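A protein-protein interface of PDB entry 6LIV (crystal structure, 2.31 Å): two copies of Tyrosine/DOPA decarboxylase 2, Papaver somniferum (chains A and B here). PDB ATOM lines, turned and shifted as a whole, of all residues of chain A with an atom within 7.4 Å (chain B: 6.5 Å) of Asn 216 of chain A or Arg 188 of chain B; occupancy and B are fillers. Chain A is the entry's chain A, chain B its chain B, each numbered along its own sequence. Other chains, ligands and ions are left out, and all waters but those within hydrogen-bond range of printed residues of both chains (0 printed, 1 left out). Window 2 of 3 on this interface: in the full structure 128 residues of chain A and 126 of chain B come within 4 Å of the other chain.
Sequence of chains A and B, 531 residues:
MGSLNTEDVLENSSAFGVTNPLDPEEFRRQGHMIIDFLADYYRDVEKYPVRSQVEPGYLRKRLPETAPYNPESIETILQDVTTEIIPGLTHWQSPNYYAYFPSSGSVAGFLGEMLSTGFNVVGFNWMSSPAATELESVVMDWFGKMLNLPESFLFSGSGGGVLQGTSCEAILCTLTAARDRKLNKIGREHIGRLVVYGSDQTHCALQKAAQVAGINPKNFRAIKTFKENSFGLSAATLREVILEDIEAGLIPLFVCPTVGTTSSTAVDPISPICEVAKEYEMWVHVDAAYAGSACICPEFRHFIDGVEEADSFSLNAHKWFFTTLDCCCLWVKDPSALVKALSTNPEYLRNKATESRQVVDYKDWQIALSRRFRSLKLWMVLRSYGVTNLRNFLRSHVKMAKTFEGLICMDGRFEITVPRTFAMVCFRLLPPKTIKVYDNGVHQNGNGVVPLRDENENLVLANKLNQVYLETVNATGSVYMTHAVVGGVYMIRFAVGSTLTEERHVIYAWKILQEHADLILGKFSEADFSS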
ATOM      1  N   ILE A 191      -2.495 -15.029   3.370  1.00  0.00           N
ATOM      2  CA  ILE A 191      -3.863 -15.523   3.236  1.00  0.00           C
ATOM      3  C   ILE A 191      -4.627 -14.731   2.182  1.00  0.00           C
ATOM      4  O   ILE A 191      -5.529 -15.265   1.526  1.00  0.00           O
ATOM      5  CB  ILE A 191      -4.581 -15.494   4.601  1.00  0.00           C
ATOM      6  CG1 ILE A 191      -5.930 -16.213   4.515  1.00  0.00           C
ATOM      7  CG2 ILE A 191      -4.760 -14.062   5.093  1.00  0.00           C
ATOM      8  CD1 ILE A 191      -6.707 -16.215   5.815  1.00  0.00           C
ATOM      9  N   GLY A 192      -4.272 -13.462   1.986  1.00  0.00           N
ATOM     10  CA  GLY A 192      -4.925 -12.637   0.988  1.00  0.00           C
ATOM     11  C   GLY A 192      -4.550 -12.941  -0.445  1.00  0.00           C
ATOM     12  O   GLY A 192      -5.076 -12.292  -1.355  1.00  0.00           O
ATOM     13  N   ARG A 193      -3.658 -13.904  -0.675  1.00  0.00           N
ATOM     14  CA  ARG A 193      -3.274 -14.307  -2.019  1.00  0.00           C
ATOM     15  C   ARG A 193      -3.761 -15.701  -2.389  1.00  0.00           C
ATOM     16  O   ARG A 193      -3.570 -16.120  -3.536  1.00  0.00           O
ATOM     17  CB  ARG A 193      -1.749 -14.249  -2.176  1.00  0.00           C
ATOM     18  CG  ARG A 193      -1.152 -12.870  -1.947  1.00  0.00           C
ATOM     19  CD  ARG A 193       0.355 -12.952  -1.775  1.00  0.00           C
ATOM     20  NE  ARG A 193       0.991 -13.638  -2.896  1.00  0.00           N
ATOM     21  CZ  ARG A 193       2.051 -14.430  -2.782  1.00  0.00           C
ATOM     22  NH1 ARG A 193       2.601 -14.638  -1.593  1.00  0.00           N
ATOM     23  NH2 ARG A 193       2.564 -15.011  -3.857  1.00  0.00           N
ATOM     24  N   LEU A 194      -4.378 -16.425  -1.459  1.00  0.00           N
ATOM     25  CA  LEU A 194      -4.839 -17.777  -1.740  1.00  0.00           C
ATOM     26  C   LEU A 194      -6.085 -17.745  -2.616  1.00  0.00           C
ATOM     27  O   LEU A 194      -6.997 -16.941  -2.402  1.00  0.00           O
ATOM     28  CB  LEU A 194      -5.129 -18.517  -0.436  1.00  0.00           C
ATOM     29  CG  LEU A 194      -3.982 -18.516   0.576  1.00  0.00           C
ATOM     30  CD1 LEU A 194      -4.348 -19.314   1.818  1.00  0.00           C
ATOM     31  CD2 LEU A 194      -2.708 -19.053  -0.057  1.00  0.00           C
ATOM     32  N   VAL A 195      -6.120 -18.631  -3.610  1.00  0.00           N
ATOM     33  CA  VAL A 195      -7.195 -18.679  -4.593  1.00  0.00           C
ATOM     34  C   VAL A 195      -7.910 -20.018  -4.475  1.00  0.00           C
ATOM     35  O   VAL A 195      -7.264 -21.067  -4.373  1.00  0.00           O
ATOM     36  CB  VAL A 195      -6.662 -18.471  -6.023  1.00  0.00           C
ATOM     37  CG1 VAL A 195      -7.812 -18.207  -6.980  1.00  0.00           C
ATOM     38  CG2 VAL A 195      -5.669 -17.324  -6.055  1.00  0.00           C
ATOM     39  N   VAL A 196      -9.239 -19.977  -4.491  1.00  0.00           N
ATOM     40  CA  VAL A 196     -10.081 -21.166  -4.441  1.00  0.00           C
ATOM     41  C   VAL A 196     -10.775 -21.303  -5.788  1.00  0.00           C
ATOM     42  O   VAL A 196     -11.347 -20.334  -6.300  1.00  0.00           O
ATOM     43  CB  VAL A 196     -11.102 -21.083  -3.292  1.00  0.00           C
ATOM     44  CG1 VAL A 196     -12.066 -22.254  -3.350  1.00  0.00           C
ATOM     45  CG2 VAL A 196     -10.384 -21.043  -1.952  1.00  0.00           C
ATOM     46  N   ALA A 210     -15.200 -20.473   1.465  1.00  0.00           N
ATOM     47  CA  ALA A 210     -14.094 -19.551   1.234  1.00  0.00           C
ATOM     48  C   ALA A 210     -14.312 -18.225   1.950  1.00  0.00           C
ATOM     49  O   ALA A 210     -13.346 -17.606   2.409  1.00  0.00           O
ATOM     50  CB  ALA A 210     -13.903 -19.322  -0.265  1.00  0.00           C
ATOM     51  N   GLN A 211     -15.563 -17.777   2.061  1.00  0.00           N
ATOM     52  CA  GLN A 211     -15.839 -16.540   2.782  1.00  0.00           C
ATOM     53  C   GLN A 211     -15.567 -16.697   4.274  1.00  0.00           C
ATOM     54  O   GLN A 211     -15.013 -15.791   4.908  1.00  0.00           O
ATOM     55  CB  GLN A 211     -17.283 -16.101   2.538  1.00  0.00           C
ATOM     56  CG  GLN A 211     -17.530 -15.558   1.138  1.00  0.00           C
ATOM     57  CD  GLN A 211     -18.987 -15.217   0.890  1.00  0.00           C
ATOM     58  OE1 GLN A 211     -19.411 -15.053  -0.255  1.00  0.00           O
ATOM     59  NE2 GLN A 211     -19.762 -15.105   1.963  1.00  0.00           N
ATOM     60  N   ALA A 213     -13.554 -19.036   5.742  1.00  0.00           N
ATOM     61  CA  ALA A 213     -12.160 -19.385   5.994  1.00  0.00           C
ATOM     62  C   ALA A 213     -11.201 -18.214   5.829  1.00  0.00           C
ATOM     63  O   ALA A 213     -10.000 -18.389   6.065  1.00  0.00           O
ATOM     64  CB  ALA A 213     -11.732 -20.528   5.073  1.00  0.00           C
ATOM     65  N   GLY A 214     -11.680 -17.040   5.431  1.00  0.00           N
ATOM     66  CA  GLY A 214     -10.818 -15.888   5.275  1.00  0.00           C
ATOM     67  C   GLY A 214     -10.248 -15.692   3.890  1.00  0.00           C
ATOM     68  O   GLY A 214      -9.408 -14.802   3.707  1.00  0.00           O
ATOM     69  N   ILE A 215     -10.664 -16.498   2.911  1.00  0.00           N
ATOM     70  CA  ILE A 215     -10.239 -16.279   1.536  1.00  0.00           C
ATOM     71  C   ILE A 215     -10.803 -14.955   1.046  1.00  0.00           C
ATOM     72  O   ILE A 215     -11.957 -14.605   1.328  1.00  0.00           O
ATOM     73  CB  ILE A 215     -10.685 -17.443   0.634  1.00  0.00           C
ATOM     74  CG1 ILE A 215     -10.141 -18.766   1.169  1.00  0.00           C
ATOM     75  CG2 ILE A 215     -10.228 -17.218  -0.802  1.00  0.00           C
ATOM     76  CD1 ILE A 215      -8.631 -18.829   1.214  1.00  0.00           C
ATOM     77  N   ASN A 216      -9.989 -14.209   0.326  1.00  0.00           N
ATOM     78  CA  ASN A 216     -10.425 -12.920  -0.182  1.00  0.00           C
ATOM     79  C   ASN A 216     -11.516 -13.120  -1.230  1.00  0.00           C
ATOM     80  O   ASN A 216     -11.373 -13.981  -2.106  1.00  0.00           O
ATOM     81  CB  ASN A 216      -9.238 -12.168  -0.767  1.00  0.00           C
ATOM     82  CG  ASN A 216      -9.545 -10.717  -1.014  1.00  0.00           C
ATOM     83  OD1 ASN A 216     -10.387 -10.392  -1.843  1.00  0.00           O
ATOM     84  ND2 ASN A 216      -8.866  -9.832  -0.297  1.00  0.00           N
ATOM     85  N   PRO A 217     -12.619 -12.361  -1.168  1.00  0.00           N
ATOM     86  CA  PRO A 217     -13.721 -12.589  -2.123  1.00  0.00           C
ATOM     87  C   PRO A 217     -13.305 -12.472  -3.578  1.00  0.00           C
ATOM     88  O   PRO A 217     -13.786 -13.242  -4.418  1.00  0.00           O
ATOM     89  CB  PRO A 217     -14.743 -11.509  -1.737  1.00  0.00           C
ATOM     90  CG  PRO A 217     -14.459 -11.217  -0.305  1.00  0.00           C
ATOM     91  CD  PRO A 217     -12.969 -11.358  -0.147  1.00  0.00           C
ATOM     92  N   LYS A 218     -12.421 -11.526  -3.902  1.00  0.00           N
ATOM     93  CA  LYS A 218     -11.942 -11.392  -5.273  1.00  0.00           C
ATOM     94  C   LYS A 218     -11.025 -12.535  -5.691  1.00  0.00           C
ATOM     95  O   LYS A 218     -10.632 -12.589  -6.861  1.00  0.00           O
ATOM     96  CB  LYS A 218     -11.233 -10.044  -5.462  1.00  0.00           C
ATOM     97  CG  LYS A 218     -12.105  -8.826  -5.146  1.00  0.00           C
ATOM     98  CD  LYS A 218     -11.758  -8.190  -3.806  1.00  0.00           C
ATOM     99  CE  LYS A 218     -12.966  -7.503  -3.176  1.00  0.00           C
ATOM    100  NZ  LYS A 218     -12.791  -7.319  -1.700  1.00  0.00           N
ATOM    101  N   ASN A 219     -10.695 -13.453  -4.781  1.00  0.00           N
ATOM    102  CA  ASN A 219      -9.864 -14.609  -5.092  1.00  0.00           C
ATOM    103  C   ASN A 219     -10.667 -15.904  -5.149  1.00  0.00           C
ATOM    104  O   ASN A 219     -10.105 -16.989  -4.972  1.00  0.00           O
ATOM    105  CB  ASN A 219      -8.727 -14.730  -4.077  1.00  0.00           C
ATOM    106  CG  ASN A 219      -7.664 -13.668  -4.267  1.00  0.00           C
ATOM    107  OD1 ASN A 219      -7.549 -13.074  -5.340  1.00  0.00           O
ATOM    108  ND2 ASN A 219      -6.877 -13.422  -3.227  1.00  0.00           N
ATOM    109  N   PHE A 220     -11.975 -15.812  -5.376  1.00  0.00           N
ATOM    110  CA  PHE A 220     -12.810 -16.977  -5.632  1.00  0.00           C
ATOM    111  C   PHE A 220     -13.070 -17.071  -7.128  1.00  0.00           C
ATOM    112  O   PHE A 220     -13.453 -16.081  -7.761  1.00  0.00           O
ATOM    113  CB  PHE A 220     -14.132 -16.895  -4.867  1.00  0.00           C
ATOM    114  CG  PHE A 220     -15.057 -18.048  -5.138  1.00  0.00           C
ATOM    115  CD1 PHE A 220     -14.872 -19.266  -4.504  1.00  0.00           C
ATOM    116  CD2 PHE A 220     -16.108 -17.918  -6.033  1.00  0.00           C
ATOM    117  CE1 PHE A 220     -15.719 -20.331  -4.753  1.00  0.00           C
ATOM    118  CE2 PHE A 220     -16.959 -18.979  -6.286  1.00  0.00           C
ATOM    119  CZ  PHE A 220     -16.764 -20.187  -5.645  1.00  0.00           C
ATOM    120  N   ARG A 221     -12.865 -18.259  -7.688  1.00  0.00           N
ATOM    121  CA  ARG A 221     -12.966 -18.478  -9.123  1.00  0.00           C
ATOM    122  C   ARG A 221     -14.157 -19.372  -9.436  1.00  0.00           C
ATOM    123  O   ARG A 221     -14.269 -20.479  -8.896  1.00  0.00           O
ATOM    124  CB  ARG A 221     -11.683 -19.105  -9.672  1.00  0.00           C
ATOM    125  CG  ARG A 221     -10.443 -18.255  -9.469  1.00  0.00           C
ATOM    126  CD  ARG A 221     -10.388 -17.100 -10.453  1.00  0.00           C
ATOM    127  NE  ARG A 221      -9.212 -16.263 -10.240  1.00  0.00           N
ATOM    128  CZ  ARG A 221      -9.187 -15.199  -9.444  1.00  0.00           C
ATOM    129  NH1 ARG A 221     -10.279 -14.840  -8.782  1.00  0.00           N
ATOM    130  NH2 ARG A 221      -8.072 -14.495  -9.310  1.00  0.00           N
ATOM    131  N   THR B 176     -17.178 -14.064  12.224  1.00  0.00           N
ATOM    132  CA  THR B 176     -17.036 -13.677  10.823  1.00  0.00           C
ATOM    133  C   THR B 176     -17.862 -12.437  10.511  1.00  0.00           C
ATOM    134  O   THR B 176     -17.454 -11.597   9.701  1.00  0.00           O
ATOM    135  CB  THR B 176     -17.441 -14.828   9.900  1.00  0.00           C
ATOM    136  OG1 THR B 176     -18.854 -15.051   9.998  1.00  0.00           O
ATOM    137  CG2 THR B 176     -16.691 -16.101  10.258  1.00  0.00           C
ATOM    138  N   ARG B 179     -15.796  -9.764  11.900  1.00  0.00           N
ATOM    139  CA  ARG B 179     -14.633  -9.605  11.033  1.00  0.00           C
ATOM    140  C   ARG B 179     -14.998  -8.859   9.756  1.00  0.00           C
ATOM    141  O   ARG B 179     -14.310  -7.913   9.357  1.00  0.00           O
ATOM    142  CB  ARG B 179     -14.040 -10.976  10.709  1.00  0.00           C
ATOM    143  CG  ARG B 179     -12.818 -10.940   9.810  1.00  0.00           C
ATOM    144  CD  ARG B 179     -12.640 -12.266   9.088  1.00  0.00           C
ATOM    145  NE  ARG B 179     -13.752 -12.540   8.182  1.00  0.00           N
ATOM    146  CZ  ARG B 179     -13.982 -13.720   7.615  1.00  0.00           C
ATOM    147  NH1 ARG B 179     -13.175 -14.744   7.858  1.00  0.00           N
ATOM    148  NH2 ARG B 179     -15.020 -13.876   6.805  1.00  0.00           N
ATOM    149  N   ASP B 180     -16.088  -9.272   9.102  1.00  0.00           N
ATOM    150  CA  ASP B 180     -16.480  -8.636   7.848  1.00  0.00           C
ATOM    151  C   ASP B 180     -16.940  -7.201   8.070  1.00  0.00           C
ATOM    152  O   ASP B 180     -16.703  -6.333   7.222  1.00  0.00           O
ATOM    153  CB  ASP B 180     -17.576  -9.454   7.165  1.00  0.00           C
ATOM    154  CG  ASP B 180     -17.018 -10.564   6.298  1.00  0.00           C
ATOM    155  OD1 ASP B 180     -15.869 -10.991   6.546  1.00  0.00           O
ATOM    156  OD2 ASP B 180     -17.722 -11.009   5.367  1.00  0.00           O
ATOM    157  N   ARG B 181     -17.598  -6.927   9.200  1.00  0.00           N
ATOM    158  CA  ARG B 181     -18.036  -5.563   9.484  1.00  0.00           C
ATOM    159  C   ARG B 181     -16.848  -4.616   9.587  1.00  0.00           C
ATOM    160  O   ARG B 181     -16.913  -3.470   9.124  1.00  0.00           O
ATOM    161  CB  ARG B 181     -18.861  -5.533  10.772  1.00  0.00           C
ATOM    162  CG  ARG B 181     -19.188  -4.131  11.266  1.00  0.00           C
ATOM    163  CD  ARG B 181     -19.830  -4.160  12.643  1.00  0.00           C
ATOM    164  NE  ARG B 181     -21.266  -4.417  12.572  1.00  0.00           N
ATOM    165  CZ  ARG B 181     -22.044  -4.606  13.633  1.00  0.00           C
ATOM    166  NH1 ARG B 181     -21.525  -4.568  14.852  1.00  0.00           N
ATOM    167  NH2 ARG B 181     -23.341  -4.834  13.475  1.00  0.00           N
ATOM    168  N   LEU B 183     -13.528  -5.370   8.419  1.00  0.00           N
ATOM    169  CA  LEU B 183     -12.685  -5.430   7.229  1.00  0.00           C
ATOM    170  C   LEU B 183     -13.336  -4.746   6.033  1.00  0.00           C
ATOM    171  O   LEU B 183     -12.630  -4.255   5.146  1.00  0.00           O
ATOM    172  CB  LEU B 183     -12.347  -6.882   6.890  1.00  0.00           C
ATOM    173  CG  LEU B 183     -11.399  -7.609   7.846  1.00  0.00           C
ATOM    174  CD1 LEU B 183     -10.935  -8.921   7.237  1.00  0.00           C
ATOM    175  CD2 LEU B 183     -10.210  -6.728   8.204  1.00  0.00           C
ATOM    176  N   ASN B 184     -14.670  -4.702   5.983  1.00  0.00           N
ATOM    177  CA  ASN B 184     -15.333  -4.001   4.890  1.00  0.00           C
ATOM    178  C   ASN B 184     -15.202  -2.491   5.016  1.00  0.00           C
ATOM    179  O   ASN B 184     -15.391  -1.779   4.023  1.00  0.00           O
ATOM    180  CB  ASN B 184     -16.810  -4.394   4.822  1.00  0.00           C
ATOM    181  CG  ASN B 184     -17.027  -5.718   4.117  1.00  0.00           C
ATOM    182  OD1 ASN B 184     -16.205  -6.141   3.304  1.00  0.00           O
ATOM    183  ND2 ASN B 184     -18.135  -6.379   4.426  1.00  0.00           N
ATOM    184  N   ILE B 186     -12.249  -1.080   6.574  1.00  0.00           N
ATOM    185  CA  ILE B 186     -10.824  -0.759   6.585  1.00  0.00           C
ATOM    186  C   ILE B 186     -10.027  -1.532   5.545  1.00  0.00           C
ATOM    187  O   ILE B 186      -8.873  -1.156   5.272  1.00  0.00           O
ATOM    188  CB  ILE B 186     -10.209  -0.982   7.983  1.00  0.00           C
ATOM    189  CG1 ILE B 186     -10.173  -2.474   8.315  1.00  0.00           C
ATOM    190  CG2 ILE B 186     -10.993  -0.212   9.038  1.00  0.00           C
ATOM    191  CD1 ILE B 186      -9.339  -2.803   9.529  1.00  0.00           C
ATOM    192  N   GLY B 187     -10.587  -2.577   4.960  1.00  0.00           N
ATOM    193  CA  GLY B 187      -9.870  -3.325   3.941  1.00  0.00           C
ATOM    194  C   GLY B 187      -9.586  -4.743   4.394  1.00  0.00           C
ATOM    195  O   GLY B 187      -9.245  -4.987   5.557  1.00  0.00           O
ATOM    196  N   ARG B 188      -9.735  -5.692   3.464  1.00  0.00           N
ATOM    197  CA  ARG B 188      -9.508  -7.101   3.772  1.00  0.00           C
ATOM    198  C   ARG B 188      -8.059  -7.402   4.131  1.00  0.00           C
ATOM    199  O   ARG B 188      -7.800  -8.386   4.834  1.00  0.00           O
ATOM    200  CB  ARG B 188      -9.920  -7.972   2.584  1.00  0.00           C
ATOM    201  CG  ARG B 188     -11.399  -7.921   2.244  1.00  0.00           C
ATOM    202  CD  ARG B 188     -12.183  -8.962   3.021  1.00  0.00           C
ATOM    203  NE  ARG B 188     -13.621  -8.749   2.904  1.00  0.00           N
ATOM    204  CZ  ARG B 188     -14.534  -9.375   3.637  1.00  0.00           C
ATOM    205  NH1 ARG B 188     -14.161 -10.264   4.548  1.00  0.00           N
ATOM    206  NH2 ARG B 188     -15.823  -9.115   3.460  1.00  0.00           N
ATOM    207  N   GLU B 189      -7.111  -6.588   3.662  1.00  0.00           N
ATOM    208  CA  GLU B 189      -5.695  -6.843   3.898  1.00  0.00           C
ATOM    209  C   GLU B 189      -5.304  -6.741   5.366  1.00  0.00           C
ATOM    210  O   GLU B 189      -4.185  -7.129   5.715  1.00  0.00           O
ATOM    211  CB  GLU B 189      -4.845  -5.873   3.073  1.00  0.00           C
ATOM    212  CG  GLU B 189      -4.970  -4.414   3.495  1.00  0.00           C
ATOM    213  CD  GLU B 189      -6.063  -3.676   2.744  1.00  0.00           C
ATOM    214  OE1 GLU B 189      -6.977  -4.338   2.208  1.00  0.00           O
ATOM    215  OE2 GLU B 189      -6.008  -2.429   2.688  1.00  0.00           O
ATOM    216  N   HIS B 190      -6.185  -6.236   6.227  1.00  0.00           N
ATOM    217  CA  HIS B 190      -5.888  -6.065   7.642  1.00  0.00           C
ATOM    218  C   HIS B 190      -6.365  -7.233   8.498  1.00  0.00           C
ATOM    219  O   HIS B 190      -6.408  -7.105   9.726  1.00  0.00           O
ATOM    220  CB  HIS B 190      -6.512  -4.767   8.158  1.00  0.00           C
ATOM    221  CG  HIS B 190      -6.014  -3.539   7.463  1.00  0.00           C
ATOM    222  ND1 HIS B 190      -4.673  -3.259   7.316  1.00  0.00           N
ATOM    223  CD2 HIS B 190      -6.679  -2.515   6.877  1.00  0.00           C
ATOM    224  CE1 HIS B 190      -4.533  -2.115   6.668  1.00  0.00           C
ATOM    225  NE2 HIS B 190      -5.735  -1.645   6.390  1.00  0.00           N
ATOM    226  N   ILE B 191      -6.725  -8.363   7.882  1.00  0.00           N
ATOM    227  CA  ILE B 191      -7.220  -9.503   8.649  1.00  0.00           C
ATOM    228  C   ILE B 191      -6.159 -10.014   9.614  1.00  0.00           C
ATOM    229  O   ILE B 191      -6.482 -10.505  10.703  1.00  0.00           O
ATOM    230  CB  ILE B 191      -7.712 -10.613   7.696  1.00  0.00           C
ATOM    231  CG1 ILE B 191      -8.407 -11.729   8.480  1.00  0.00           C
ATOM    232  CG2 ILE B 191      -6.563 -11.166   6.860  1.00  0.00           C
ATOM    233  CD1 ILE B 191      -9.157 -12.712   7.604  1.00  0.00           C
ATOM    234  N   GLY B 192      -4.882  -9.889   9.251  1.00  0.00           N
ATOM    235  CA  GLY B 192      -3.796 -10.320  10.110  1.00  0.00           C
ATOM    236  C   GLY B 192      -3.512  -9.416  11.288  1.00  0.00           C
ATOM    237  O   GLY B 192      -2.597  -9.708  12.066  1.00  0.00           O
ATOM    238  N   LYS B 340     -24.488 -10.239   5.697  1.00  0.00           N
ATOM    239  CA  LYS B 340     -23.424  -9.636   4.900  1.00  0.00           C
ATOM    240  C   LYS B 340     -22.191 -10.529   4.838  1.00  0.00           C
ATOM    241  O   LYS B 340     -21.461 -10.514   3.840  1.00  0.00           O
ATOM    242  CB  LYS B 340     -23.063  -8.261   5.468  1.00  0.00           C
ATOM    243  CG  LYS B 340     -21.902  -7.565   4.770  1.00  0.00           C
ATOM    244  CD  LYS B 340     -22.334  -6.937   3.455  1.00  0.00           C
ATOM    245  CE  LYS B 340     -21.364  -5.849   3.016  1.00  0.00           C
ATOM    246  NZ  LYS B 340     -21.280  -4.745   4.012  1.00  0.00           N
ATOM    247  N   ALA B 341     -21.946 -11.319   5.881  1.00  0.00           N
ATOM    248  CA  ALA B 341     -20.758 -12.161   5.928  1.00  0.00           C
ATOM    249  C   ALA B 341     -21.010 -13.584   5.452  1.00  0.00           C
ATOM    250  O   ALA B 341     -20.094 -14.218   4.918  1.00  0.00           O
ATOM    251  CB  ALA B 341     -20.192 -12.197   7.351  1.00  0.00           C
ATOM    252  N   ARG B 350     -26.693  -8.167  -0.821  1.00  0.00           N
ATOM    253  CA  ARG B 350     -26.475  -8.571   0.567  1.00  0.00           C
ATOM    254  C   ARG B 350     -26.844  -7.477   1.562  1.00  0.00           C
ATOM    255  O   ARG B 350     -27.726  -7.662   2.401  1.00  0.00           O
ATOM    256  CB  ARG B 350     -25.014  -8.971   0.775  1.00  0.00           C
ATOM    257  CG  ARG B 350     -24.799 -10.447   1.059  1.00  0.00           C
ATOM    258  CD  ARG B 350     -23.324 -10.749   1.262  1.00  0.00           C
ATOM    259  NE  ARG B 350     -22.764 -11.515   0.153  1.00  0.00           N
ATOM    260  CZ  ARG B 350     -21.515 -11.964   0.116  1.00  0.00           C
ATOM    261  NH1 ARG B 350     -20.692 -11.724   1.129  1.00  0.00           N
ATOM    262  NH2 ARG B 350     -21.089 -12.655  -0.933  1.00  0.00           N
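OE1 of Gln 211 of chain A is in hydrogen-bond range of NH2 of Arg 350 of chain B, at 3.0 Å. The backbone carbonyl oxygen (O) of Gln 211 of chain A sits at hydrogen-bond distance from the guanidinium group (NH2) of Arg 179 of chain B (2.7 Å). O of Ala 341 of chain B is in hydrogen-bond range of NE2 of Gln 211 of chain A (3.1 Å).
O of Lys 340 of chain B sits at hydrogen-bond distance from NH1 of Arg 350 of chain B (3.1 Å). The side-chain carboxylate (OD1) of Asp 180 of chain B is in salt-bridge range of the guanidinium group (NH2) of Arg 179 of chain B. The guanidinium group of Arg 188 of chain B lies within hydrogen-bond range of the side-chain amide oxygen of Asn 184 of chain B (3.0 Å). The side-chain carboxylate of Asp 180 of chain B is in salt-bridge range of the guanidinium group of Arg 188 of chain B (2.7 Å). OD1 of Asn 216 of chain A lies within hydrogen-bond range of N of Lys 218 of chain A (3.1 Å).
Among the printed residues, pairs that only touch across the chains: Ile 191 of chain A with Ile 191 of chain B, Gly 214 of chain A with Arg 179 of chain B and Asn 216 of chain A with Arg 188 of chain B.
Of the printed residues of chain B, Gln 211 of chain A touches Arg 179 (2.7 Å), Ala 341 (3.1 Å) and Arg 350 (3.0 Å). Of the printed residues of chain B, Gly 214 of chain A touches Arg 179 (3.7 Å). Asn 216 of chain A touches just one residue of chain B: Arg 188. Lys 218 of chain A touches none of the printed residues of chain B. Phe 220 of chain A touches none of the printed residues of chain B. Of chain A, only Asn 216 comes within 4 Å of Arg 188 of chain B. Of the printed residues of chain A, Ile 191 of chain B touches Ile 191. Printed residues of chain A within 4 Å of Ala 341 of chain B: Gln 211.
Of the 16 printed residues of chain B, 5 touch a printed residue of chain A. Printed residues of chain B that touch a printed residue of chain A: Arg 179, Arg 188, Ile 191, Ala 341 and Arg 350. Of the 17 printed residues of chain A, 4 touch a printed residue of chain B. Among the printed residues, 6 pairs touch across the chains. Among the printed residues, no Asp or Glu carboxylate lies within 4 Å of a Lys or Arg side-chain nitrogen of the other chain.
Ile 191 of chain A touches its own counterpart, Ile 191 of chain B. 2 positions are printed for both chains.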
